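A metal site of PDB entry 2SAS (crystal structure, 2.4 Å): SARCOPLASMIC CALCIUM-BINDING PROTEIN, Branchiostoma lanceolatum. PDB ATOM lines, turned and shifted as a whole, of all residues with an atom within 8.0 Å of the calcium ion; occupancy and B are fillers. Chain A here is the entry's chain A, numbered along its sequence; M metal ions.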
ATOM      1  N   PHE A  14      -2.859 -10.220  13.239  1.00  0.00           N
ATOM      2  CA  PHE A  14      -2.079 -10.672  12.050  1.00  0.00           C
ATOM      3  C   PHE A  14      -0.662 -10.904  12.577  1.00  0.00           C
ATOM      4  O   PHE A  14      -0.101 -11.990  12.528  1.00  0.00           O
ATOM      5  CB  PHE A  14      -2.176  -9.635  10.922  1.00  0.00           C
ATOM      6  CG  PHE A  14      -1.544  -9.898   9.600  1.00  0.00           C
ATOM      7  CD1 PHE A  14      -2.187 -10.650   8.616  1.00  0.00           C
ATOM      8  CD2 PHE A  14      -0.291  -9.400   9.304  1.00  0.00           C
ATOM      9  CE1 PHE A  14      -1.586 -10.930   7.393  1.00  0.00           C
ATOM     10  CE2 PHE A  14       0.345  -9.633   8.099  1.00  0.00           C
ATOM     11  CZ  PHE A  14      -0.329 -10.405   7.163  1.00  0.00           C
ATOM     12  N   LEU A  18      -0.258 -14.638  14.051  1.00  0.00           N
ATOM     13  CA  LEU A  18      -0.110 -15.473  12.835  1.00  0.00           C
ATOM     14  C   LEU A  18       1.214 -15.312  12.092  1.00  0.00           C
ATOM     15  O   LEU A  18       1.745 -16.381  11.723  1.00  0.00           O
ATOM     16  CB  LEU A  18      -1.300 -15.259  11.888  1.00  0.00           C
ATOM     17  CG  LEU A  18      -2.634 -15.870  12.249  1.00  0.00           C
ATOM     18  CD1 LEU A  18      -3.734 -15.009  11.633  1.00  0.00           C
ATOM     19  CD2 LEU A  18      -2.768 -17.305  11.725  1.00  0.00           C
ATOM     20  N   ASP A  19       1.631 -14.095  11.897  1.00  0.00           N
ATOM     21  CA  ASP A  19       2.872 -13.777  11.175  1.00  0.00           C
ATOM     22  C   ASP A  19       4.051 -13.921  12.124  1.00  0.00           C
ATOM     23  O   ASP A  19       4.697 -12.944  12.547  1.00  0.00           O
ATOM     24  CB  ASP A  19       2.762 -12.416  10.459  1.00  0.00           C
ATOM     25  CG  ASP A  19       3.973 -12.108   9.605  1.00  0.00           C
ATOM     26  OD1 ASP A  19       4.568 -13.060   9.049  1.00  0.00           O
ATOM     27  OD2 ASP A  19       4.406 -10.936   9.472  1.00  0.00           O
ATOM     28  N   MET A  20       4.344 -15.172  12.434  1.00  0.00           N
ATOM     29  CA  MET A  20       5.444 -15.532  13.380  1.00  0.00           C
ATOM     30  C   MET A  20       6.802 -15.035  12.907  1.00  0.00           C
ATOM     31  O   MET A  20       7.555 -14.530  13.742  1.00  0.00           O
ATOM     32  CB  MET A  20       5.482 -17.022  13.610  1.00  0.00           C
ATOM     33  CG  MET A  20       4.153 -17.523  14.050  1.00  0.00           C
ATOM     34  SD  MET A  20       3.886 -16.921  15.770  1.00  0.00           S
ATOM     35  CE  MET A  20       2.944 -15.434  15.458  1.00  0.00           C
ATOM     36  N   ASN A  21       7.067 -15.159  11.604  1.00  0.00           N
ATOM     37  CA  ASN A  21       8.341 -14.727  11.053  1.00  0.00           C
ATOM     38  C   ASN A  21       8.385 -13.262  10.673  1.00  0.00           C
ATOM     39  O   ASN A  21       9.380 -12.886  10.012  1.00  0.00           O
ATOM     40  CB  ASN A  21       8.791 -15.600   9.878  1.00  0.00           C
ATOM     41  CG  ASN A  21       7.826 -15.557   8.709  1.00  0.00           C
ATOM     42  OD1 ASN A  21       7.197 -14.518   8.469  1.00  0.00           O
ATOM     43  ND2 ASN A  21       7.729 -16.676   7.963  1.00  0.00           N
ATOM     44  N   HIS A  22       7.350 -12.496  10.931  1.00  0.00           N
ATOM     45  CA  HIS A  22       7.377 -11.055  10.629  1.00  0.00           C
ATOM     46  C   HIS A  22       7.640 -10.570   9.258  1.00  0.00           C
ATOM     47  O   HIS A  22       8.345  -9.528   9.081  1.00  0.00           O
ATOM     48  CB  HIS A  22       8.412 -10.411  11.678  1.00  0.00           C
ATOM     49  CG  HIS A  22       7.778 -10.649  13.037  1.00  0.00           C
ATOM     50  ND1 HIS A  22       8.275 -11.427  14.059  1.00  0.00           N
ATOM     51  CD2 HIS A  22       6.528 -10.217  13.421  1.00  0.00           C
ATOM     52  CE1 HIS A  22       7.357 -11.463  15.008  1.00  0.00           C
ATOM     53  NE2 HIS A  22       6.291 -10.739  14.662  1.00  0.00           N
ATOM     54  N   ASP A  23       7.090 -11.116   8.184  1.00  0.00           N
ATOM     55  CA  ASP A  23       7.375 -10.587   6.830  1.00  0.00           C
ATOM     56  C   ASP A  23       6.191  -9.911   6.196  1.00  0.00           C
ATOM     57  O   ASP A  23       6.249  -9.514   5.002  1.00  0.00           O
ATOM     58  CB  ASP A  23       8.035 -11.700   6.010  1.00  0.00           C
ATOM     59  CG  ASP A  23       7.086 -12.861   5.813  1.00  0.00           C
ATOM     60  OD1 ASP A  23       5.992 -12.816   6.468  1.00  0.00           O
ATOM     61  OD2 ASP A  23       7.367 -13.762   5.006  1.00  0.00           O
ATOM     62  N   GLY A  24       5.088  -9.682   6.914  1.00  0.00           N
ATOM     63  CA  GLY A  24       3.920  -9.000   6.423  1.00  0.00           C
ATOM     64  C   GLY A  24       2.975  -9.898   5.651  1.00  0.00           C
ATOM     65  O   GLY A  24       2.051  -9.369   4.980  1.00  0.00           O
ATOM     66  N   SER A  25       3.241 -11.183   5.713  1.00  0.00           N
ATOM     67  CA  SER A  25       2.454 -12.205   5.014  1.00  0.00           C
ATOM     68  C   SER A  25       2.368 -13.444   5.963  1.00  0.00           C
ATOM     69  O   SER A  25       3.350 -13.681   6.641  1.00  0.00           O
ATOM     70  CB  SER A  25       3.154 -12.772   3.820  1.00  0.00           C
ATOM     71  OG  SER A  25       3.074 -12.289   2.555  1.00  0.00           O
ATOM     72  N   ILE A  26       1.251 -14.108   5.838  1.00  0.00           N
ATOM     73  CA  ILE A  26       0.914 -15.336   6.496  1.00  0.00           C
ATOM     74  C   ILE A  26       1.240 -16.402   5.394  1.00  0.00           C
ATOM     75  O   ILE A  26       0.777 -16.183   4.274  1.00  0.00           O
ATOM     76  CB  ILE A  26      -0.557 -15.586   6.955  1.00  0.00           C
ATOM     77  CG1 ILE A  26      -1.234 -14.383   7.659  1.00  0.00           C
ATOM     78  CG2 ILE A  26      -0.582 -16.799   7.936  1.00  0.00           C
ATOM     79  CD1 ILE A  26      -0.359 -13.686   8.714  1.00  0.00           C
ATOM     80  N   GLN A  27       1.956 -17.435   5.764  1.00  0.00           N
ATOM     81  CA  GLN A  27       2.327 -18.504   4.803  1.00  0.00           C
ATOM     82  C   GLN A  27       2.594 -19.769   5.610  1.00  0.00           C
ATOM     83  O   GLN A  27       2.815 -19.474   6.808  1.00  0.00           O
ATOM     84  CB  GLN A  27       3.680 -18.127   4.137  1.00  0.00           C
ATOM     85  CG  GLN A  27       3.519 -16.901   3.237  1.00  0.00           C
ATOM     86  CD  GLN A  27       4.879 -16.556   2.677  1.00  0.00           C
ATOM     87  OE1 GLN A  27       5.444 -15.490   2.977  1.00  0.00           O
ATOM     88  NE2 GLN A  27       5.323 -17.489   1.878  1.00  0.00           N
ATOM     89  N   ASP A  28       2.596 -20.950   5.052  1.00  0.00           N
ATOM     90  CA  ASP A  28       2.890 -22.166   5.815  1.00  0.00           C
ATOM     91  C   ASP A  28       4.119 -21.966   6.719  1.00  0.00           C
ATOM     92  O   ASP A  28       4.106 -22.425   7.849  1.00  0.00           O
ATOM     93  CB  ASP A  28       3.081 -23.430   4.960  1.00  0.00           C
ATOM     94  CG  ASP A  28       3.576 -24.651   5.693  1.00  0.00           C
ATOM     95  OD1 ASP A  28       2.868 -25.316   6.484  1.00  0.00           O
ATOM     96  OD2 ASP A  28       4.773 -25.011   5.507  1.00  0.00           O
ATOM     97  N   ASN A  29       5.155 -21.300   6.269  1.00  0.00           N
ATOM     98  CA  ASN A  29       6.331 -21.139   7.097  1.00  0.00           C
ATOM     99  C   ASN A  29       6.031 -20.499   8.449  1.00  0.00           C
ATOM    100  O   ASN A  29       6.835 -20.719   9.401  1.00  0.00           O
ATOM    101  CB  ASN A  29       7.501 -20.531   6.357  1.00  0.00           C
ATOM    102  CG  ASN A  29       7.399 -19.046   6.058  1.00  0.00           C
ATOM    103  OD1 ASN A  29       6.295 -18.494   5.988  1.00  0.00           O
ATOM    104  ND2 ASN A  29       8.549 -18.391   5.896  1.00  0.00           N
ATOM    105  N   ASP A  30       5.017 -19.699   8.540  1.00  0.00           N
ATOM    106  CA  ASP A  30       4.614 -19.019   9.782  1.00  0.00           C
ATOM    107  C   ASP A  30       4.129 -20.145  10.748  1.00  0.00           C
ATOM    108  O   ASP A  30       4.562 -20.134  11.898  1.00  0.00           O
ATOM    109  CB  ASP A  30       3.515 -17.998   9.529  1.00  0.00           C
ATOM    110  CG  ASP A  30       4.065 -16.762   8.863  1.00  0.00           C
ATOM    111  OD1 ASP A  30       5.059 -16.224   9.368  1.00  0.00           O
ATOM    112  OD2 ASP A  30       3.507 -16.397   7.813  1.00  0.00           O
ATOM    113  N   PHE A  31       3.335 -21.023  10.206  1.00  0.00           N
ATOM    114  CA  PHE A  31       2.803 -22.190  10.913  1.00  0.00           C
ATOM    115  C   PHE A  31       3.931 -23.154  11.317  1.00  0.00           C
ATOM    116  O   PHE A  31       3.895 -23.775  12.400  1.00  0.00           O
ATOM    117  CB  PHE A  31       1.674 -22.846  10.089  1.00  0.00           C
ATOM    118  CG  PHE A  31       0.461 -21.949   9.982  1.00  0.00           C
ATOM    119  CD1 PHE A  31       0.431 -20.862   9.124  1.00  0.00           C
ATOM    120  CD2 PHE A  31      -0.627 -22.138  10.851  1.00  0.00           C
ATOM    121  CE1 PHE A  31      -0.647 -19.996   9.066  1.00  0.00           C
ATOM    122  CE2 PHE A  31      -1.743 -21.297  10.822  1.00  0.00           C
ATOM    123  CZ  PHE A  31      -1.740 -20.238   9.906  1.00  0.00           C
ATOM    124  N   ASP A  33       6.791 -22.250  12.147  1.00  0.00           N
ATOM    125  CA  ASP A  33       7.392 -21.458  13.231  1.00  0.00           C
ATOM    126  C   ASP A  33       6.618 -21.636  14.535  1.00  0.00           C
ATOM    127  O   ASP A  33       7.097 -21.432  15.666  1.00  0.00           O
ATOM    128  CB  ASP A  33       7.440 -19.976  12.884  1.00  0.00           C
ATOM    129  CG  ASP A  33       8.569 -19.474  12.046  1.00  0.00           C
ATOM    130  OD1 ASP A  33       9.112 -20.308  11.270  1.00  0.00           O
ATOM    131  OD2 ASP A  33       8.906 -18.267  12.076  1.00  0.00           O
ATOM    132  N   VAL A  76      -0.111 -17.436  -0.237  1.00  0.00           N
ATOM    133  CA  VAL A  76       0.373 -16.386   0.683  1.00  0.00           C
ATOM    134  C   VAL A  76      -0.890 -15.608   1.076  1.00  0.00           C
ATOM    135  O   VAL A  76      -1.680 -15.303   0.148  1.00  0.00           O
ATOM    136  CB  VAL A  76       1.402 -15.485   0.010  1.00  0.00           C
ATOM    137  CG1 VAL A  76       2.000 -14.464   0.991  1.00  0.00           C
ATOM    138  CG2 VAL A  76       2.500 -16.244  -0.718  1.00  0.00           C
ATOM    139  N   VAL A  77      -1.117 -15.374   2.365  1.00  0.00           N
ATOM    140  CA  VAL A  77      -2.289 -14.548   2.731  1.00  0.00           C
ATOM    141  C   VAL A  77      -1.645 -13.180   3.039  1.00  0.00           C
ATOM    142  O   VAL A  77      -0.746 -13.109   3.915  1.00  0.00           O
ATOM    143  CB  VAL A  77      -3.147 -15.099   3.843  1.00  0.00           C
ATOM    144  CG1 VAL A  77      -4.176 -14.086   4.357  1.00  0.00           C
ATOM    145  CG2 VAL A  77      -3.866 -16.408   3.508  1.00  0.00           C
HETATM  146 CA    CA M   1       5.024 -14.601   7.546  1.00  0.00          CA
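The calcium ion is bound by the backbone carbonyl oxygen (O) of Ser 25, the side-chain carboxylate (OD1) of Asp 19, the side-chain carboxylate (OD1) of Asp 23, the side-chain amide oxygen (OD1) of Asn 21, the side-chain carboxylate (OD2) of Asp 30 and the side-chain carboxylate (OD1) of Asp 30.
The backbone carbonyl oxygen (O) of Asp 19 sits close to a ring nitrogen (NE2) of His 22, at 3.4 Å. The backbone NH (N) of Gly 24 lies within hydrogen-bond range of the side-chain carboxylate (OD2) of Asp 19 (2.9 Å). The backbone NH (N) of Asp 19 lies within hydrogen-bond range of the backbone carbonyl oxygen (O) of Phe 14 (2.8 Å). OD2 of Asp 23 sits close to OE1 of Gln 27 (3.3 Å). ND2 of Asn 29 lies close to ND2 of Asn 21, 2.8 Å away. The backbone NH of Gln 27 lies close to the side-chain carboxylate of Asp 30, 2.8 Å away. OD1 of Asp 30 lies close to N of Met 20 (3.3 Å).
Of the 18 residues printed, 5 come within 4 Å of the calcium ion.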
